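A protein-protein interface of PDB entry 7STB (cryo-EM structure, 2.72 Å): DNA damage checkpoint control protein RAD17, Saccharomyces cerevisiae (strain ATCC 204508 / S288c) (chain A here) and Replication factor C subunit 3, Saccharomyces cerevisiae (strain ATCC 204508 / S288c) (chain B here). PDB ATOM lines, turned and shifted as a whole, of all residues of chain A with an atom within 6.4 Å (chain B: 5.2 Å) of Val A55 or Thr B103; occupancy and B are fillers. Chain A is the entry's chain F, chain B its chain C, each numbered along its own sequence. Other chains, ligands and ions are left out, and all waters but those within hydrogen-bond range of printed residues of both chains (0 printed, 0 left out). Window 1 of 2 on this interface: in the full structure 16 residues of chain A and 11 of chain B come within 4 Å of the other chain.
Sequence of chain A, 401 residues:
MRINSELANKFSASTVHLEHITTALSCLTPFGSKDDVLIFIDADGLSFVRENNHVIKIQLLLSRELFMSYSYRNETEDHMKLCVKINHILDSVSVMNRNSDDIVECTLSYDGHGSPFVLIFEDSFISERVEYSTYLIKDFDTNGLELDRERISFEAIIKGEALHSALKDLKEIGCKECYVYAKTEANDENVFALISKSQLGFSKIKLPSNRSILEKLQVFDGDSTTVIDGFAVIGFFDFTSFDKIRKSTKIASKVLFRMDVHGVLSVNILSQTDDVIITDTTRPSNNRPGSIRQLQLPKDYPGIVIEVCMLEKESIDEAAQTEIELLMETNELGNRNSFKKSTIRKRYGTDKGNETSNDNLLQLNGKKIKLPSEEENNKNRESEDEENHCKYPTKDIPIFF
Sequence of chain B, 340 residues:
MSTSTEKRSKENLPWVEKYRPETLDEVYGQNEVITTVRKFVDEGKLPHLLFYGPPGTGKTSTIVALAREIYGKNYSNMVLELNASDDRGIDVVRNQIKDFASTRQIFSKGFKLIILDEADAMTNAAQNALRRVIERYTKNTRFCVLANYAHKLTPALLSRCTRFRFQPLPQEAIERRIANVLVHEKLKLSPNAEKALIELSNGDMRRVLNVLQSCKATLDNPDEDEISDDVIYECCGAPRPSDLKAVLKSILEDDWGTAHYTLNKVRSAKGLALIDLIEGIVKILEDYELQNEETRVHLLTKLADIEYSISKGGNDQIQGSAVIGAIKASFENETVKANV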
ATOM      1  N   GLU A  51      -1.442  21.296 -21.972  1.00  0.00           N
ATOM      2  CA  GLU A  51      -0.871  20.055 -22.479  1.00  0.00           C
ATOM      3  C   GLU A  51      -1.732  19.559 -23.630  1.00  0.00           C
ATOM      4  O   GLU A  51      -2.961  19.533 -23.522  1.00  0.00           O
ATOM      5  CB  GLU A  51      -0.778  18.992 -21.377  1.00  0.00           C
ATOM      6  CG  GLU A  51      -2.117  18.585 -20.769  1.00  0.00           C
ATOM      7  CD  GLU A  51      -2.822  17.488 -21.552  1.00  0.00           C
ATOM      8  OE1 GLU A  51      -2.149  16.778 -22.329  1.00  0.00           O
ATOM      9  OE2 GLU A  51      -4.050  17.337 -21.388  1.00  0.00           O
ATOM     10  N   ASN A  52      -1.089  19.174 -24.730  1.00  0.00           N
ATOM     11  CA  ASN A  52      -1.786  18.734 -25.929  1.00  0.00           C
ATOM     12  C   ASN A  52      -1.223  17.396 -26.388  1.00  0.00           C
ATOM     13  O   ASN A  52       0.002  17.220 -26.476  1.00  0.00           O
ATOM     14  CB  ASN A  52      -1.672  19.779 -27.043  1.00  0.00           C
ATOM     15  CG  ASN A  52      -2.553  19.460 -28.232  1.00  0.00           C
ATOM     16  OD1 ASN A  52      -3.240  18.440 -28.254  1.00  0.00           O
ATOM     17  ND2 ASN A  52      -2.547  20.341 -29.223  1.00  0.00           N
ATOM     18  N   ASN A  53      -2.136  16.457 -26.656  1.00  0.00           N
ATOM     19  CA  ASN A  53      -1.846  15.130 -27.197  1.00  0.00           C
ATOM     20  C   ASN A  53      -0.875  14.340 -26.329  1.00  0.00           C
ATOM     21  O   ASN A  53      -0.298  13.350 -26.785  1.00  0.00           O
ATOM     22  CB  ASN A  53      -1.311  15.228 -28.632  1.00  0.00           C
ATOM     23  CG  ASN A  53      -2.397  15.559 -29.636  1.00  0.00           C
ATOM     24  OD1 ASN A  53      -3.557  15.184 -29.463  1.00  0.00           O
ATOM     25  ND2 ASN A  53      -2.025  16.266 -30.696  1.00  0.00           N
ATOM     26  N   HIS A  54      -0.690  14.745 -25.074  1.00  0.00           N
ATOM     27  CA  HIS A  54       0.283  14.128 -24.177  1.00  0.00           C
ATOM     28  C   HIS A  54       1.692  14.157 -24.759  1.00  0.00           C
ATOM     29  O   HIS A  54       2.578  13.443 -24.280  1.00  0.00           O
ATOM     30  CB  HIS A  54      -0.108  12.684 -23.840  1.00  0.00           C
ATOM     31  CG  HIS A  54      -1.352  12.570 -23.016  1.00  0.00           C
ATOM     32  ND1 HIS A  54      -1.742  11.391 -22.420  1.00  0.00           N
ATOM     33  CD2 HIS A  54      -2.292  13.487 -22.685  1.00  0.00           C
ATOM     34  CE1 HIS A  54      -2.870  11.585 -21.760  1.00  0.00           C
ATOM     35  NE2 HIS A  54      -3.224  12.849 -21.905  1.00  0.00           N
ATOM     36  N   VAL A  55       1.915  14.976 -25.785  1.00  0.00           N
ATOM     37  CA  VAL A  55       3.219  15.063 -26.427  1.00  0.00           C
ATOM     38  C   VAL A  55       3.800  16.467 -26.402  1.00  0.00           C
ATOM     39  O   VAL A  55       5.018  16.615 -26.591  1.00  0.00           O
ATOM     40  CB  VAL A  55       3.162  14.544 -27.880  1.00  0.00           C
ATOM     41  CG1 VAL A  55       2.744  13.082 -27.913  1.00  0.00           C
ATOM     42  CG2 VAL A  55       2.230  15.401 -28.720  1.00  0.00           C
ATOM     43  N   ILE A  56       2.998  17.511 -26.184  1.00  0.00           N
ATOM     44  CA  ILE A  56       3.539  18.859 -26.068  1.00  0.00           C
ATOM     45  C   ILE A  56       2.918  19.540 -24.858  1.00  0.00           C
ATOM     46  O   ILE A  56       1.763  19.286 -24.506  1.00  0.00           O
ATOM     47  CB  ILE A  56       3.306  19.686 -27.355  1.00  0.00           C
ATOM     48  CG1 ILE A  56       4.047  21.020 -27.277  1.00  0.00           C
ATOM     49  CG2 ILE A  56       1.827  19.913 -27.589  1.00  0.00           C
ATOM     50  CD1 ILE A  56       4.214  21.697 -28.617  1.00  0.00           C
ATOM     51  N   LYS A  57       3.704  20.390 -24.195  1.00  0.00           N
ATOM     52  CA  LYS A  57       3.194  21.167 -23.076  1.00  0.00           C
ATOM     53  C   LYS A  57       3.837  22.544 -23.094  1.00  0.00           C
ATOM     54  O   LYS A  57       4.996  22.701 -23.494  1.00  0.00           O
ATOM     55  CB  LYS A  57       3.460  20.493 -21.714  1.00  0.00           C
ATOM     56  CG  LYS A  57       4.924  20.353 -21.300  1.00  0.00           C
ATOM     57  CD  LYS A  57       5.368  21.586 -20.496  1.00  0.00           C
ATOM     58  CE  LYS A  57       6.783  21.479 -19.953  1.00  0.00           C
ATOM     59  NZ  LYS A  57       7.168  22.701 -19.201  1.00  0.00           N
ATOM     60  N   LEU A 145       5.787  15.546 -18.323  1.00  0.00           N
ATOM     61  CA  LEU A 145       6.732  15.819 -19.401  1.00  0.00           C
ATOM     62  C   LEU A 145       7.719  16.877 -18.923  1.00  0.00           C
ATOM     63  O   LEU A 145       7.339  18.027 -18.683  1.00  0.00           O
ATOM     64  CB  LEU A 145       5.997  16.278 -20.659  1.00  0.00           C
ATOM     65  CG  LEU A 145       6.858  16.539 -21.896  1.00  0.00           C
ATOM     66  CD1 LEU A 145       7.555  15.269 -22.356  1.00  0.00           C
ATOM     67  CD2 LEU A 145       6.007  17.117 -23.017  1.00  0.00           C
ATOM     68  N   SER A 241       2.990  19.909 -33.693  1.00  0.00           N
ATOM     69  CA  SER A 241       3.456  20.319 -32.374  1.00  0.00           C
ATOM     70  C   SER A 241       4.510  21.417 -32.465  1.00  0.00           C
ATOM     71  O   SER A 241       4.552  22.313 -31.615  1.00  0.00           O
ATOM     72  CB  SER A 241       4.013  19.111 -31.621  1.00  0.00           C
ATOM     73  OG  SER A 241       2.968  18.263 -31.178  1.00  0.00           O
ATOM     74  N   LYS A 244       3.325  25.172 -32.708  1.00  0.00           N
ATOM     75  CA  LYS A 244       2.588  25.748 -31.592  1.00  0.00           C
ATOM     76  C   LYS A 244       3.420  26.728 -30.773  1.00  0.00           C
ATOM     77  O   LYS A 244       2.879  27.352 -29.855  1.00  0.00           O
ATOM     78  CB  LYS A 244       2.063  24.634 -30.684  1.00  0.00           C
ATOM     79  CG  LYS A 244       0.864  23.898 -31.259  1.00  0.00           C
ATOM     80  CD  LYS A 244       0.614  22.584 -30.543  1.00  0.00           C
ATOM     81  CE  LYS A 244      -0.433  21.752 -31.268  1.00  0.00           C
ATOM     82  NZ  LYS A 244      -0.281  20.298 -30.993  1.00  0.00           N
ATOM     83  N   CYS A 309       7.832  22.010 -23.740  1.00  0.00           N
ATOM     84  CA  CYS A 309       8.457  20.708 -23.937  1.00  0.00           C
ATOM     85  C   CYS A 309       7.666  19.923 -24.969  1.00  0.00           C
ATOM     86  O   CYS A 309       6.448  19.764 -24.833  1.00  0.00           O
ATOM     87  CB  CYS A 309       8.541  19.908 -22.634  1.00  0.00           C
ATOM     88  SG  CYS A 309       9.879  20.417 -21.532  1.00  0.00           S
ATOM     89  N   MET A 310       8.359  19.422 -25.988  1.00  0.00           N
ATOM     90  CA  MET A 310       7.737  18.602 -27.017  1.00  0.00           C
ATOM     91  C   MET A 310       8.552  17.335 -27.227  1.00  0.00           C
ATOM     92  O   MET A 310       9.773  17.326 -27.059  1.00  0.00           O
ATOM     93  CB  MET A 310       7.591  19.365 -28.345  1.00  0.00           C
ATOM     94  CG  MET A 310       8.895  19.613 -29.083  1.00  0.00           C
ATOM     95  SD  MET A 310       8.673  20.590 -30.582  1.00  0.00           S
ATOM     96  CE  MET A 310       8.055  22.132 -29.915  1.00  0.00           C
ATOM     97  N   LEU A 311       7.860  16.261 -27.594  1.00  0.00           N
ATOM     98  CA  LEU A 311       8.481  14.958 -27.767  1.00  0.00           C
ATOM     99  C   LEU A 311       8.996  14.784 -29.191  1.00  0.00           C
ATOM    100  O   LEU A 311       8.634  15.523 -30.109  1.00  0.00           O
ATOM    101  CB  LEU A 311       7.489  13.843 -27.437  1.00  0.00           C
ATOM    102  CG  LEU A 311       7.297  13.516 -25.955  1.00  0.00           C
ATOM    103  CD1 LEU A 311       6.074  12.631 -25.766  1.00  0.00           C
ATOM    104  CD2 LEU A 311       8.538  12.849 -25.372  1.00  0.00           C
ATOM    105  N   GLU A 312       9.850  13.780 -29.362  1.00  0.00           N
ATOM    106  CA  GLU A 312      10.415  13.425 -30.654  1.00  0.00           C
ATOM    107  C   GLU A 312       9.694  12.202 -31.210  1.00  0.00           C
ATOM    108  O   GLU A 312       9.178  11.371 -30.459  1.00  0.00           O
ATOM    109  CB  GLU A 312      11.916  13.151 -30.527  1.00  0.00           C
ATOM    110  CG  GLU A 312      12.515  12.319 -31.649  1.00  0.00           C
ATOM    111  CD  GLU A 312      14.025  12.230 -31.564  1.00  0.00           C
ATOM    112  OE1 GLU A 312      14.596  12.713 -30.564  1.00  0.00           O
ATOM    113  OE2 GLU A 312      14.642  11.673 -32.497  1.00  0.00           O
ATOM    114  N   LYS A 313       9.656  12.105 -32.536  1.00  0.00           N
ATOM    115  CA  LYS A 313       8.954  11.008 -33.181  1.00  0.00           C
ATOM    116  C   LYS A 313       9.671   9.682 -32.927  1.00  0.00           C
ATOM    117  O   LYS A 313      10.876   9.631 -32.674  1.00  0.00           O
ATOM    118  CB  LYS A 313       8.830  11.256 -34.683  1.00  0.00           C
ATOM    119  CG  LYS A 313       8.072  12.526 -35.057  1.00  0.00           C
ATOM    120  CD  LYS A 313       6.610  12.487 -34.621  1.00  0.00           C
ATOM    121  CE  LYS A 313       5.777  11.554 -35.484  1.00  0.00           C
ATOM    122  NZ  LYS A 313       5.727  11.987 -36.907  1.00  0.00           N
ATOM    123  N   GLU A 314       8.901   8.596 -33.024  1.00  0.00           N
ATOM    124  CA  GLU A 314       9.381   7.296 -32.564  1.00  0.00           C
ATOM    125  C   GLU A 314      10.615   6.842 -33.336  1.00  0.00           C
ATOM    126  O   GLU A 314      11.572   6.333 -32.740  1.00  0.00           O
ATOM    127  CB  GLU A 314       8.260   6.261 -32.679  1.00  0.00           C
ATOM    128  CG  GLU A 314       8.565   4.923 -32.013  1.00  0.00           C
ATOM    129  CD  GLU A 314       9.373   3.990 -32.895  1.00  0.00           C
ATOM    130  OE1 GLU A 314       9.256   4.088 -34.134  1.00  0.00           O
ATOM    131  OE2 GLU A 314      10.130   3.161 -32.347  1.00  0.00           O
ATOM    132  N   SER A 315      10.619   7.013 -34.656  1.00  0.00           N
ATOM    133  CA  SER A 315      11.715   6.514 -35.475  1.00  0.00           C
ATOM    134  C   SER A 315      11.917   7.425 -36.676  1.00  0.00           C
ATOM    135  O   SER A 315      11.069   8.258 -37.005  1.00  0.00           O
ATOM    136  CB  SER A 315      11.459   5.073 -35.933  1.00  0.00           C
ATOM    137  OG  SER A 315      10.305   4.995 -36.751  1.00  0.00           O
ATOM    138  N   ASP B  99      -0.390  10.476 -33.617  1.00  0.00           N
ATOM    139  CA  ASP B  99       0.637  11.284 -32.969  1.00  0.00           C
ATOM    140  C   ASP B  99       1.123  10.628 -31.685  1.00  0.00           C
ATOM    141  O   ASP B  99       2.326  10.619 -31.403  1.00  0.00           O
ATOM    142  CB  ASP B  99       0.097  12.685 -32.682  1.00  0.00           C
ATOM    143  CG  ASP B  99      -0.259  13.444 -33.945  1.00  0.00           C
ATOM    144  OD1 ASP B  99       0.139  12.997 -35.042  1.00  0.00           O
ATOM    145  OD2 ASP B  99      -0.936  14.488 -33.842  1.00  0.00           O
ATOM    146  N   PHE B 100       0.205  10.075 -30.889  1.00  0.00           N
ATOM    147  CA  PHE B 100       0.617   9.443 -29.640  1.00  0.00           C
ATOM    148  C   PHE B 100       1.500   8.228 -29.896  1.00  0.00           C
ATOM    149  O   PHE B 100       2.510   8.030 -29.211  1.00  0.00           O
ATOM    150  CB  PHE B 100      -0.605   9.044 -28.816  1.00  0.00           C
ATOM    151  CG  PHE B 100      -0.263   8.510 -27.454  1.00  0.00           C
ATOM    152  CD1 PHE B 100       0.349   9.320 -26.511  1.00  0.00           C
ATOM    153  CD2 PHE B 100      -0.549   7.199 -27.116  1.00  0.00           C
ATOM    154  CE1 PHE B 100       0.668   8.833 -25.259  1.00  0.00           C
ATOM    155  CE2 PHE B 100      -0.232   6.706 -25.865  1.00  0.00           C
ATOM    156  CZ  PHE B 100       0.376   7.524 -24.936  1.00  0.00           C
ATOM    157  N   ALA B 101       1.139   7.404 -30.880  1.00  0.00           N
ATOM    158  CA  ALA B 101       1.854   6.160 -31.130  1.00  0.00           C
ATOM    159  C   ALA B 101       3.152   6.354 -31.901  1.00  0.00           C
ATOM    160  O   ALA B 101       3.958   5.420 -31.960  1.00  0.00           O
ATOM    161  CB  ALA B 101       0.953   5.186 -31.893  1.00  0.00           C
ATOM    162  N   SER B 102       3.378   7.529 -32.485  1.00  0.00           N
ATOM    163  CA  SER B 102       4.557   7.784 -33.302  1.00  0.00           C
ATOM    164  C   SER B 102       5.592   8.649 -32.594  1.00  0.00           C
ATOM    165  O   SER B 102       6.476   9.202 -33.257  1.00  0.00           O
ATOM    166  CB  SER B 102       4.146   8.442 -34.621  1.00  0.00           C
ATOM    167  OG  SER B 102       3.496   9.680 -34.394  1.00  0.00           O
ATOM    168  N   THR B 103       5.509   8.779 -31.274  1.00  0.00           N
ATOM    169  CA  THR B 103       6.441   9.582 -30.497  1.00  0.00           C
ATOM    170  C   THR B 103       7.241   8.697 -29.550  1.00  0.00           C
ATOM    171  O   THR B 103       6.796   7.624 -29.137  1.00  0.00           O
ATOM    172  CB  THR B 103       5.704  10.666 -29.702  1.00  0.00           C
ATOM    173  OG1 THR B 103       4.664  10.070 -28.919  1.00  0.00           O
ATOM    174  CG2 THR B 103       5.111  11.707 -30.639  1.00  0.00           C
ATOM    175  N   ARG B 104       8.440   9.165 -29.213  1.00  0.00           N
ATOM    176  CA  ARG B 104       9.337   8.406 -28.357  1.00  0.00           C
ATOM    177  C   ARG B 104       8.788   8.350 -26.932  1.00  0.00           C
ATOM    178  O   ARG B 104       7.714   8.873 -26.623  1.00  0.00           O
ATOM    179  CB  ARG B 104      10.737   9.013 -28.381  1.00  0.00           C
ATOM    180  CG  ARG B 104      11.389   8.985 -29.759  1.00  0.00           C
ATOM    181  CD  ARG B 104      12.889   9.296 -29.746  1.00  0.00           C
ATOM    182  NE  ARG B 104      13.614   8.709 -28.625  1.00  0.00           N
ATOM    183  CZ  ARG B 104      14.935   8.681 -28.521  1.00  0.00           C
ATOM    184  NH1 ARG B 104      15.715   9.193 -29.458  1.00  0.00           N
ATOM    185  NH2 ARG B 104      15.489   8.121 -27.449  1.00  0.00           N
ATOM    186  N   GLN B 105       9.545   7.701 -26.054  1.00  0.00           N
ATOM    187  CA  GLN B 105       9.111   7.422 -24.695  1.00  0.00           C
ATOM    188  C   GLN B 105       9.667   8.465 -23.732  1.00  0.00           C
ATOM    189  O   GLN B 105      10.754   9.010 -23.935  1.00  0.00           O
ATOM    190  CB  GLN B 105       9.566   6.027 -24.266  1.00  0.00           C
ATOM    191  CG  GLN B 105       8.740   5.438 -23.147  1.00  0.00           C
ATOM    192  CD  GLN B 105       7.373   5.007 -23.628  1.00  0.00           C
ATOM    193  OE1 GLN B 105       6.394   5.737 -23.486  1.00  0.00           O
ATOM    194  NE2 GLN B 105       7.301   3.819 -24.211  1.00  0.00           N
ATOM    195  N   LYS B 112       4.201   2.319 -24.982  1.00  0.00           N
ATOM    196  CA  LYS B 112       3.052   3.182 -24.753  1.00  0.00           C
ATOM    197  C   LYS B 112       1.780   2.385 -24.998  1.00  0.00           C
ATOM    198  O   LYS B 112       1.652   1.715 -26.026  1.00  0.00           O
ATOM    199  CB  LYS B 112       3.095   4.408 -25.667  1.00  0.00           C
ATOM    200  CG  LYS B 112       4.365   5.230 -25.539  1.00  0.00           C
ATOM    201  CD  LYS B 112       4.479   6.272 -26.640  1.00  0.00           C
ATOM    202  CE  LYS B 112       3.614   7.485 -26.357  1.00  0.00           C
ATOM    203  NZ  LYS B 112       3.928   8.614 -27.273  1.00  0.00           N
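The backbone carbonyl oxygen (O) of Ser B102 lies within hydrogen-bond range of the backbone NH (N) of Glu A314, at 2.5 Å.
NH1 of Arg B104 lies within salt-bridge range of OE1 of Glu A312, at 3.9 Å.
The backbone carbonyl oxygen (O) of Asp B99 lies within hydrogen-bond range of the side-chain hydroxyl (OG) of Ser B102 (3.3 Å).
O of Asp B99 lies close to OG1 of Thr B103, at 3.5 Å.
The side-chain hydroxyl of Thr B103 sits at hydrogen-bond distance from the backbone carbonyl oxygen of Phe B100 (3.0 Å).
OD1 of Asn A52 lies close to ND2 of Asn A53, 3.5 Å away.
N of Leu A311 sits at hydrogen-bond distance from O of Val A55 (3.0 Å).
OG of Ser A315 is in hydrogen-bond range of OE1 of Glu A314 (3.0 Å).
Among the printed residues, pairs that only touch across the chains: Asn A53 with Asp B99 (3.8 Å), Val A55 with Thr B103 (3.7 Å), Glu A312 with Thr B103 (3.3 Å), Lys A313 with Ser B102 (3.1 Å), Lys A313 with Thr B103 (3.9 Å), Lys A313 with Arg B104 (3.0 Å), Glu A314 with Thr B103 (3.7 Å) and Glu A314 with Arg B104 (3.8 Å).
Printed residues of chain B within 4 Å of Asn A53: Asp B99 (3.8 Å).
Val A55 touches just one residue of chain B: Thr B103.
Ile A56 touches none of the printed residues of chain B.
Of the printed residues of chain B, Glu A312 touches Thr B103 (3.3 Å) and Arg B104 (2.6 Å).
Printed residues of chain B within 4 Å of Lys A313: Ser B102, Thr B103 and Arg B104.
Of the printed residues of chain B, Glu A314 touches Ser B102 (2.5 Å), Thr B103 (3.7 Å) and Arg B104 (3.8 Å).
Of chain A, only Val A55, Glu A312, Lys A313 and Glu A314 come within 4 Å of Thr B103.
Of the printed residues of chain A, Arg B104 touches Glu A312 (2.6 Å), Lys A313 (3.0 Å) and Glu A314 (3.8 Å).
The nearest residue of chain B that does not touch Val A55 is Asp B99 (4.3 Å).
The nearest residue of chain A that does not touch Thr B103 is Leu A311 (4.3 Å).
Among the printed residues, 10 pairs touch across the chains.
Among the printed residues, Asp or Glu carboxylates within 4 Å of a Lys or Arg side-chain nitrogen of the other chain: Glu A312 with Arg B104 (3.9 Å).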
